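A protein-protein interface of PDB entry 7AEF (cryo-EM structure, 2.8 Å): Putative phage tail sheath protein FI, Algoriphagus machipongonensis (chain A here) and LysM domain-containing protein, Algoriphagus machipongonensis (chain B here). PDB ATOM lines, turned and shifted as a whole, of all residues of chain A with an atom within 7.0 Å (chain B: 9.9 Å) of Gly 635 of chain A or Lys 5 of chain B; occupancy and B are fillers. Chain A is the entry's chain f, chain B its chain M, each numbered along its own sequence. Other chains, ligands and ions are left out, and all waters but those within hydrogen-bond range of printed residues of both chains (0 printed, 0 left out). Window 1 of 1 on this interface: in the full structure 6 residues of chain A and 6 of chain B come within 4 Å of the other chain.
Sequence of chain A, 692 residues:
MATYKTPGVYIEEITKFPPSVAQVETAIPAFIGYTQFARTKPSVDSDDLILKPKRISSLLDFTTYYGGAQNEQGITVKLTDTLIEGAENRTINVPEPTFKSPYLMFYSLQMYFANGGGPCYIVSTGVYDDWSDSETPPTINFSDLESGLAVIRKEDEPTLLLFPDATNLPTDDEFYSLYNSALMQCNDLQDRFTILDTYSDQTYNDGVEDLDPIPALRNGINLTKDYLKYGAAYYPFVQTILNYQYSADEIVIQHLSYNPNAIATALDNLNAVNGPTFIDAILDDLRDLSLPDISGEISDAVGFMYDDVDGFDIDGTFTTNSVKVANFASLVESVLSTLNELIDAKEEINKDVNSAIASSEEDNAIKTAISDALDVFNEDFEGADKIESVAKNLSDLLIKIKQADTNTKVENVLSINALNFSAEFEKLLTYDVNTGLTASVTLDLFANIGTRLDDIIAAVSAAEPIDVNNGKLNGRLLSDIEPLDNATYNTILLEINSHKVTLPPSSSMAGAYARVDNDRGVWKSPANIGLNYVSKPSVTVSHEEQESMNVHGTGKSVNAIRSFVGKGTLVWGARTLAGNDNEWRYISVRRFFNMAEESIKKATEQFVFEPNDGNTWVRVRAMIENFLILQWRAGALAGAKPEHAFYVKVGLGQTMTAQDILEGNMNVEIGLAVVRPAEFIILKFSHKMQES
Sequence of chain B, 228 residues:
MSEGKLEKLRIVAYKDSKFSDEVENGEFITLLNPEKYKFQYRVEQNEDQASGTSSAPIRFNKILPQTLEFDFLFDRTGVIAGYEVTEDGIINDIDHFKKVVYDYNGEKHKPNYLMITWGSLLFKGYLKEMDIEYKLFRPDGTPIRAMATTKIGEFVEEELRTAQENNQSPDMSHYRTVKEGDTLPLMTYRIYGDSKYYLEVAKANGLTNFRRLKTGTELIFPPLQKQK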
ATOM      1  N   ARG A 520      -7.481 -12.824 -13.420  1.00  0.00           N
ATOM      2  CA  ARG A 520      -7.183 -13.211 -12.049  1.00  0.00           C
ATOM      3  C   ARG A 520      -5.950 -12.548 -11.446  1.00  0.00           C
ATOM      4  O   ARG A 520      -5.920 -12.297 -10.241  1.00  0.00           O
ATOM      5  CB  ARG A 520      -7.013 -14.715 -11.977  1.00  0.00           C
ATOM      6  CG  ARG A 520      -8.256 -15.531 -12.320  1.00  0.00           C
ATOM      7  CD  ARG A 520      -9.314 -15.405 -11.286  1.00  0.00           C
ATOM      8  NE  ARG A 520     -10.490 -16.188 -11.618  1.00  0.00           N
ATOM      9  CZ  ARG A 520     -11.534 -15.761 -12.349  1.00  0.00           C
ATOM     10  NH1 ARG A 520     -11.583 -14.534 -12.862  1.00  0.00           N
ATOM     11  NH2 ARG A 520     -12.546 -16.588 -12.564  1.00  0.00           N
ATOM     12  N   TRP A 523      -0.283 -13.915 -10.325  1.00  0.00           N
ATOM     13  CA  TRP A 523      -0.011 -15.046  -9.454  1.00  0.00           C
ATOM     14  C   TRP A 523      -0.867 -16.272  -9.762  1.00  0.00           C
ATOM     15  O   TRP A 523      -0.727 -17.300  -9.098  1.00  0.00           O
ATOM     16  CB  TRP A 523      -0.194 -14.629  -7.999  1.00  0.00           C
ATOM     17  CG  TRP A 523      -1.495 -13.978  -7.719  1.00  0.00           C
ATOM     18  CD1 TRP A 523      -2.649 -14.575  -7.364  1.00  0.00           C
ATOM     19  CD2 TRP A 523      -1.765 -12.594  -7.770  1.00  0.00           C
ATOM     20  NE1 TRP A 523      -3.618 -13.650  -7.188  1.00  0.00           N
ATOM     21  CE2 TRP A 523      -3.097 -12.425  -7.435  1.00  0.00           C
ATOM     22  CE3 TRP A 523      -0.997 -11.479  -8.067  1.00  0.00           C
ATOM     23  CZ2 TRP A 523      -3.683 -11.198  -7.383  1.00  0.00           C
ATOM     24  CZ3 TRP A 523      -1.575 -10.247  -8.020  1.00  0.00           C
ATOM     25  CH2 TRP A 523      -2.899 -10.109  -7.683  1.00  0.00           C
ATOM     26  N   LEU A 630      -1.163  -4.379   0.344  1.00  0.00           N
ATOM     27  CA  LEU A 630      -2.161  -4.443  -0.709  1.00  0.00           C
ATOM     28  C   LEU A 630      -2.090  -5.761  -1.458  1.00  0.00           C
ATOM     29  O   LEU A 630      -3.125  -6.350  -1.776  1.00  0.00           O
ATOM     30  CB  LEU A 630      -1.973  -3.294  -1.685  1.00  0.00           C
ATOM     31  CG  LEU A 630      -2.299  -1.892  -1.179  1.00  0.00           C
ATOM     32  CD1 LEU A 630      -1.820  -0.890  -2.186  1.00  0.00           C
ATOM     33  CD2 LEU A 630      -3.793  -1.735  -0.967  1.00  0.00           C
ATOM     34  N   GLN A 631      -0.873  -6.252  -1.719  1.00  0.00           N
ATOM     35  CA  GLN A 631      -0.714  -7.524  -2.418  1.00  0.00           C
ATOM     36  C   GLN A 631      -1.256  -8.676  -1.592  1.00  0.00           C
ATOM     37  O   GLN A 631      -1.833  -9.628  -2.131  1.00  0.00           O
ATOM     38  CB  GLN A 631       0.757  -7.764  -2.750  1.00  0.00           C
ATOM     39  CG  GLN A 631       1.298  -6.814  -3.770  1.00  0.00           C
ATOM     40  CD  GLN A 631       0.600  -6.970  -5.067  1.00  0.00           C
ATOM     41  OE1 GLN A 631       0.507  -8.074  -5.594  1.00  0.00           O
ATOM     42  NE2 GLN A 631       0.079  -5.886  -5.595  1.00  0.00           N
ATOM     43  N   TRP A 632      -1.093  -8.581  -0.277  1.00  0.00           N
ATOM     44  CA  TRP A 632      -1.624  -9.583   0.626  1.00  0.00           C
ATOM     45  C   TRP A 632      -3.149  -9.611   0.581  1.00  0.00           C
ATOM     46  O   TRP A 632      -3.745 -10.674   0.407  1.00  0.00           O
ATOM     47  CB  TRP A 632      -1.075  -9.344   2.025  1.00  0.00           C
ATOM     48  CG  TRP A 632      -1.628 -10.206   3.070  1.00  0.00           C
ATOM     49  CD1 TRP A 632      -1.389 -11.524   3.268  1.00  0.00           C
ATOM     50  CD2 TRP A 632      -2.472  -9.798   4.127  1.00  0.00           C
ATOM     51  NE1 TRP A 632      -2.057 -11.956   4.359  1.00  0.00           N
ATOM     52  CE2 TRP A 632      -2.720 -10.908   4.907  1.00  0.00           C
ATOM     53  CE3 TRP A 632      -3.039  -8.592   4.489  1.00  0.00           C
ATOM     54  CZ2 TRP A 632      -3.504 -10.859   6.006  1.00  0.00           C
ATOM     55  CZ3 TRP A 632      -3.820  -8.540   5.603  1.00  0.00           C
ATOM     56  CH2 TRP A 632      -4.049  -9.653   6.342  1.00  0.00           C
ATOM     57  N   ARG A 633      -3.798  -8.448   0.656  1.00  0.00           N
ATOM     58  CA  ARG A 633      -5.259  -8.409   0.613  1.00  0.00           C
ATOM     59  C   ARG A 633      -5.795  -8.935  -0.713  1.00  0.00           C
ATOM     60  O   ARG A 633      -6.850  -9.573  -0.757  1.00  0.00           O
ATOM     61  CB  ARG A 633      -5.771  -6.990   0.813  1.00  0.00           C
ATOM     62  CG  ARG A 633      -5.468  -6.343   2.158  1.00  0.00           C
ATOM     63  CD  ARG A 633      -6.171  -6.944   3.318  1.00  0.00           C
ATOM     64  NE  ARG A 633      -7.604  -6.706   3.296  1.00  0.00           N
ATOM     65  CZ  ARG A 633      -8.472  -7.199   4.189  1.00  0.00           C
ATOM     66  NH1 ARG A 633      -8.058  -7.967   5.178  1.00  0.00           N
ATOM     67  NH2 ARG A 633      -9.757  -6.915   4.083  1.00  0.00           N
ATOM     68  N   ALA A 634      -5.051  -8.702  -1.793  1.00  0.00           N
ATOM     69  CA  ALA A 634      -5.389  -9.139  -3.142  1.00  0.00           C
ATOM     70  C   ALA A 634      -5.309 -10.650  -3.338  1.00  0.00           C
ATOM     71  O   ALA A 634      -5.777 -11.147  -4.362  1.00  0.00           O
ATOM     72  CB  ALA A 634      -4.463  -8.480  -4.149  1.00  0.00           C
ATOM     73  N   GLY A 635      -4.678 -11.381  -2.420  1.00  0.00           N
ATOM     74  CA  GLY A 635      -4.537 -12.817  -2.557  1.00  0.00           C
ATOM     75  C   GLY A 635      -3.226 -13.319  -3.156  1.00  0.00           C
ATOM     76  O   GLY A 635      -3.154 -14.482  -3.551  1.00  0.00           O
ATOM     77  N   ALA A 636      -2.196 -12.482  -3.265  1.00  0.00           N
ATOM     78  CA  ALA A 636      -0.938 -12.968  -3.824  1.00  0.00           C
ATOM     79  C   ALA A 636      -0.062 -13.634  -2.770  1.00  0.00           C
ATOM     80  O   ALA A 636       0.645 -14.613  -3.049  1.00  0.00           O
ATOM     81  CB  ALA A 636      -0.185 -11.820  -4.450  1.00  0.00           C
ATOM     82  N   LEU A 637      -0.083 -13.082  -1.564  1.00  0.00           N
ATOM     83  CA  LEU A 637       0.771 -13.540  -0.483  1.00  0.00           C
ATOM     84  C   LEU A 637      -0.006 -14.413   0.481  1.00  0.00           C
ATOM     85  O   LEU A 637      -1.202 -14.235   0.697  1.00  0.00           O
ATOM     86  CB  LEU A 637       1.400 -12.361   0.273  1.00  0.00           C
ATOM     87  CG  LEU A 637       2.276 -11.358  -0.533  1.00  0.00           C
ATOM     88  CD1 LEU A 637       2.743 -10.236   0.387  1.00  0.00           C
ATOM     89  CD2 LEU A 637       3.479 -12.063  -1.151  1.00  0.00           C
ATOM     90  N   ALA A 638       0.700 -15.368   1.046  1.00  0.00           N
ATOM     91  CA  ALA A 638       0.185 -16.319   2.022  1.00  0.00           C
ATOM     92  C   ALA A 638       0.255 -15.746   3.435  1.00  0.00           C
ATOM     93  O   ALA A 638       1.010 -14.828   3.676  1.00  0.00           O
ATOM     94  CB  ALA A 638       0.989 -17.603   1.928  1.00  0.00           C
ATOM     95  N   GLY A 639      -0.525 -16.299   4.368  1.00  0.00           N
ATOM     96  CA  GLY A 639      -0.459 -15.881   5.787  1.00  0.00           C
ATOM     97  C   GLY A 639      -1.751 -15.304   6.348  1.00  0.00           C
ATOM     98  O   GLY A 639      -2.394 -14.457   5.735  1.00  0.00           O
ATOM     99  N   VAL A 675       1.682 -17.817  -2.433  1.00  0.00           N
ATOM    100  CA  VAL A 675       0.689 -18.844  -2.720  1.00  0.00           C
ATOM    101  C   VAL A 675       1.114 -19.741  -3.882  1.00  0.00           C
ATOM    102  O   VAL A 675       1.542 -19.251  -4.926  1.00  0.00           O
ATOM    103  CB  VAL A 675      -0.651 -18.163  -3.016  1.00  0.00           C
ATOM    104  CG1 VAL A 675      -1.701 -19.175  -3.434  1.00  0.00           C
ATOM    105  CG2 VAL A 675      -1.092 -17.393  -1.769  1.00  0.00           C
ATOM    106  N   SER B   2      -4.104 -17.876   1.806  1.00  0.00           N
ATOM    107  CA  SER B   2      -5.114 -17.075   1.126  1.00  0.00           C
ATOM    108  C   SER B   2      -6.293 -16.787   2.042  1.00  0.00           C
ATOM    109  O   SER B   2      -7.388 -16.488   1.575  1.00  0.00           O
ATOM    110  CB  SER B   2      -5.592 -17.781  -0.141  1.00  0.00           C
ATOM    111  OG  SER B   2      -6.818 -17.237  -0.597  1.00  0.00           O
ATOM    112  N   GLU B   3      -6.052 -16.925   3.343  1.00  0.00           N
ATOM    113  CA  GLU B   3      -7.008 -16.506   4.357  1.00  0.00           C
ATOM    114  C   GLU B   3      -7.155 -14.995   4.356  1.00  0.00           C
ATOM    115  O   GLU B   3      -8.257 -14.460   4.527  1.00  0.00           O
ATOM    116  CB  GLU B   3      -6.557 -16.977   5.739  1.00  0.00           C
ATOM    117  CG  GLU B   3      -7.545 -16.677   6.848  1.00  0.00           C
ATOM    118  CD  GLU B   3      -7.096 -17.195   8.200  1.00  0.00           C
ATOM    119  OE1 GLU B   3      -7.732 -16.854   9.218  1.00  0.00           O
ATOM    120  OE2 GLU B   3      -6.047 -17.875   8.253  1.00  0.00           O
ATOM    121  N   GLY B   4      -6.034 -14.301   4.162  1.00  0.00           N
ATOM    122  CA  GLY B   4      -5.965 -12.860   4.210  1.00  0.00           C
ATOM    123  C   GLY B   4      -6.568 -12.149   3.027  1.00  0.00           C
ATOM    124  O   GLY B   4      -6.631 -10.919   3.028  1.00  0.00           O
ATOM    125  N   LYS B   5      -7.012 -12.889   2.019  1.00  0.00           N
ATOM    126  CA  LYS B   5      -7.635 -12.301   0.845  1.00  0.00           C
ATOM    127  C   LYS B   5      -9.091 -11.955   1.118  1.00  0.00           C
ATOM    128  O   LYS B   5      -9.853 -12.789   1.610  1.00  0.00           O
ATOM    129  CB  LYS B   5      -7.548 -13.267  -0.333  1.00  0.00           C
ATOM    130  CG  LYS B   5      -8.223 -12.759  -1.581  1.00  0.00           C
ATOM    131  CD  LYS B   5      -8.487 -13.862  -2.569  1.00  0.00           C
ATOM    132  CE  LYS B   5      -9.286 -13.340  -3.742  1.00  0.00           C
ATOM    133  NZ  LYS B   5      -9.465 -14.376  -4.791  1.00  0.00           N
ATOM    134  N   LEU B   6      -9.476 -10.726   0.781  1.00  0.00           N
ATOM    135  CA  LEU B   6     -10.871 -10.296   0.811  1.00  0.00           C
ATOM    136  C   LEU B   6     -11.572 -10.823  -0.437  1.00  0.00           C
ATOM    137  O   LEU B   6     -11.335 -10.337  -1.544  1.00  0.00           O
ATOM    138  CB  LEU B   6     -10.965  -8.776   0.894  1.00  0.00           C
ATOM    139  CG  LEU B   6     -12.369  -8.170   1.029  1.00  0.00           C
ATOM    140  CD1 LEU B   6     -13.009  -8.563   2.337  1.00  0.00           C
ATOM    141  CD2 LEU B   6     -12.328  -6.665   0.905  1.00  0.00           C
ATOM    142  N   GLU B   7     -12.445 -11.807  -0.260  1.00  0.00           N
ATOM    143  CA  GLU B   7     -13.176 -12.383  -1.378  1.00  0.00           C
ATOM    144  C   GLU B   7     -14.339 -11.482  -1.784  1.00  0.00           C
ATOM    145  O   GLU B   7     -14.967 -10.833  -0.946  1.00  0.00           O
ATOM    146  CB  GLU B   7     -13.683 -13.778  -1.005  1.00  0.00           C
ATOM    147  CG  GLU B   7     -14.235 -14.598  -2.165  1.00  0.00           C
ATOM    148  CD  GLU B   7     -13.151 -15.222  -3.035  1.00  0.00           C
ATOM    149  OE1 GLU B   7     -13.463 -15.636  -4.165  1.00  0.00           O
ATOM    150  OE2 GLU B   7     -11.990 -15.307  -2.591  1.00  0.00           O
ATOM    151  N   LYS B   8     -14.618 -11.440  -3.084  1.00  0.00           N
ATOM    152  CA  LYS B   8     -15.673 -10.619  -3.659  1.00  0.00           C
ATOM    153  C   LYS B   8     -16.778 -11.502  -4.222  1.00  0.00           C
ATOM    154  O   LYS B   8     -16.517 -12.598  -4.721  1.00  0.00           O
ATOM    155  CB  LYS B   8     -15.106  -9.717  -4.751  1.00  0.00           C
ATOM    156  CG  LYS B   8     -14.262  -8.586  -4.215  1.00  0.00           C
ATOM    157  CD  LYS B   8     -15.133  -7.520  -3.593  1.00  0.00           C
ATOM    158  CE  LYS B   8     -14.344  -6.650  -2.653  1.00  0.00           C
ATOM    159  NZ  LYS B   8     -13.165  -6.057  -3.319  1.00  0.00           N
ATOM    160  N   LEU B   9     -18.015 -11.014  -4.143  1.00  0.00           N
ATOM    161  CA  LEU B   9     -19.184 -11.788  -4.550  1.00  0.00           C
ATOM    162  C   LEU B   9     -19.264 -11.892  -6.073  1.00  0.00           C
ATOM    163  O   LEU B   9     -18.924 -10.952  -6.790  1.00  0.00           O
ATOM    164  CB  LEU B   9     -20.440 -11.138  -3.958  1.00  0.00           C
ATOM    165  CG  LEU B   9     -21.884 -11.389  -4.402  1.00  0.00           C
ATOM    166  CD1 LEU B   9     -22.234 -12.830  -4.358  1.00  0.00           C
ATOM    167  CD2 LEU B   9     -22.823 -10.649  -3.503  1.00  0.00           C
ATOM    168  N   ARG B  10     -19.642 -13.070  -6.568  1.00  0.00           N
ATOM    169  CA  ARG B  10     -19.759 -13.358  -7.992  1.00  0.00           C
ATOM    170  C   ARG B  10     -21.121 -13.898  -8.376  1.00  0.00           C
ATOM    171  O   ARG B  10     -21.749 -14.594  -7.610  1.00  0.00           O
ATOM    172  CB  ARG B  10     -18.781 -14.428  -8.411  1.00  0.00           C
ATOM    173  CG  ARG B  10     -17.348 -14.010  -8.473  1.00  0.00           C
ATOM    174  CD  ARG B  10     -16.569 -14.872  -9.446  1.00  0.00           C
ATOM    175  NE  ARG B  10     -16.955 -16.272  -9.384  1.00  0.00           N
ATOM    176  CZ  ARG B  10     -16.722 -17.155 -10.349  1.00  0.00           C
ATOM    177  NH1 ARG B  10     -16.119 -16.783 -11.452  1.00  0.00           N
ATOM    178  NH2 ARG B  10     -17.115 -18.402 -10.216  1.00  0.00           N
ATOM    179  N   ILE B  29     -18.655  -9.817 -11.472  1.00  0.00           N
ATOM    180  CA  ILE B  29     -17.929  -9.730 -10.210  1.00  0.00           C
ATOM    181  C   ILE B  29     -18.110  -8.320  -9.671  1.00  0.00           C
ATOM    182  O   ILE B  29     -17.873  -7.346 -10.390  1.00  0.00           O
ATOM    183  CB  ILE B  29     -16.433 -10.062 -10.374  1.00  0.00           C
ATOM    184  CG1 ILE B  29     -16.244 -11.412 -11.062  1.00  0.00           C
ATOM    185  CG2 ILE B  29     -15.735 -10.087  -9.032  1.00  0.00           C
ATOM    186  CD1 ILE B  29     -14.874 -11.624 -11.621  1.00  0.00           C
ATOM    187  N   ASN B  33     -18.636  -5.381  -1.742  1.00  0.00           N
ATOM    188  CA  ASN B  33     -19.490  -6.404  -1.161  1.00  0.00           C
ATOM    189  C   ASN B  33     -20.700  -5.776  -0.478  1.00  0.00           C
ATOM    190  O   ASN B  33     -20.621  -4.654   0.027  1.00  0.00           O
ATOM    191  CB  ASN B  33     -18.703  -7.216  -0.134  1.00  0.00           C
ATOM    192  CG  ASN B  33     -17.941  -8.359  -0.753  1.00  0.00           C
ATOM    193  OD1 ASN B  33     -18.457  -9.058  -1.608  1.00  0.00           O
ATOM    194  ND2 ASN B  33     -16.707  -8.552  -0.324  1.00  0.00           N
ATOM    195  N   TRP B 118     -20.539 -16.522  -2.631  1.00  0.00           N
ATOM    196  CA  TRP B 118     -19.648 -15.661  -1.857  1.00  0.00           C
ATOM    197  C   TRP B 118     -19.323 -16.370  -0.552  1.00  0.00           C
ATOM    198  O   TRP B 118     -20.172 -16.435   0.337  1.00  0.00           O
ATOM    199  CB  TRP B 118     -20.283 -14.304  -1.583  1.00  0.00           C
ATOM    200  CG  TRP B 118     -19.461 -13.397  -0.716  1.00  0.00           C
ATOM    201  CD1 TRP B 118     -18.107 -13.274  -0.711  1.00  0.00           C
ATOM    202  CD2 TRP B 118     -19.948 -12.477   0.261  1.00  0.00           C
ATOM    203  NE1 TRP B 118     -17.717 -12.350   0.217  1.00  0.00           N
ATOM    204  CE2 TRP B 118     -18.830 -11.843   0.827  1.00  0.00           C
ATOM    205  CE3 TRP B 118     -21.223 -12.130   0.718  1.00  0.00           C
ATOM    206  CZ2 TRP B 118     -18.944 -10.884   1.828  1.00  0.00           C
ATOM    207  CZ3 TRP B 118     -21.333 -11.174   1.707  1.00  0.00           C
ATOM    208  CH2 TRP B 118     -20.201 -10.562   2.252  1.00  0.00           C
ATOM    209  N   GLY B 119     -18.099 -16.873  -0.433  1.00  0.00           N
ATOM    210  CA  GLY B 119     -17.682 -17.547   0.783  1.00  0.00           C
ATOM    211  C   GLY B 119     -18.414 -18.855   0.989  1.00  0.00           C
ATOM    212  O   GLY B 119     -18.293 -19.792   0.199  1.00  0.00           O
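Among the printed residues, merely in contact across the chains: Arg 633 of chain A with Lys 5 of chain B, Trp 632 of chain A with Gly 4 of chain B, Arg 633 of chain A with Gly 4 of chain B, Arg 520 of chain A with Arg 10 of chain B, Gly 635 of chain A with Lys 5 of chain B and Gly 639 of chain A with Gly 4 of chain B.
The side-chain amino group (NZ) of Lys 5 of chain B lies within salt-bridge range of the side-chain carboxylate (OE2) of Glu 7 of chain B (3.5 Å).
The indole nitrogen (NE1) of Trp 632 of chain A is in hydrogen-bond range of the backbone carbonyl oxygen (O) of Gly 639 of chain A, at 2.9 Å.
The backbone NH (N) of Leu 6 of chain B lies within hydrogen-bond range of the backbone carbonyl oxygen (O) of Arg 633 of chain A, 3.3 Å away.
Of the 13 printed residues of chain A, 5 touch a printed residue of chain B.
Hydrophobic or aromatic side chains of chain A that line the printed part of chain B: Trp 632.
Printed residues of chain B that touch a printed residue of chain A: Gly 4, Lys 5, Leu 6 and Arg 10.
Hydrophobic or aromatic side chains of chain B that line the printed part of chain A: Leu 6.
Among the printed residues, no Asp or Glu carboxylate lies within 4 Å of a Lys or Arg side-chain nitrogen of the other chain.
Of the printed residues of chain B, Arg 520 of chain A touches Arg 10 (3.7 Å).
Of the printed residues of chain B, Arg 633 of chain A touches Gly 4 (3.7 Å), Lys 5 (3.3 Å) and Leu 6 (3.3 Å).
Gly 635 of chain A touches just one residue of chain B: Lys 5 (3.8 Å).
No residue of chain B comes within 4 Å of Ala 636 of chain A.
Ser 2 of chain B touches none of the printed residues of chain A.
Gly 4 of chain B touches three residues of chain A.
Of the printed residues of chain A, Lys 5 of chain B touches Arg 633 (3.3 Å) and Gly 635 (3.8 Å).
Glu 7 of chain B touches none of the printed residues of chain A.
The nearest residue of chain B that does not touch Gly 635 of chain A is Ser 2 of chain B (5.3 Å).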
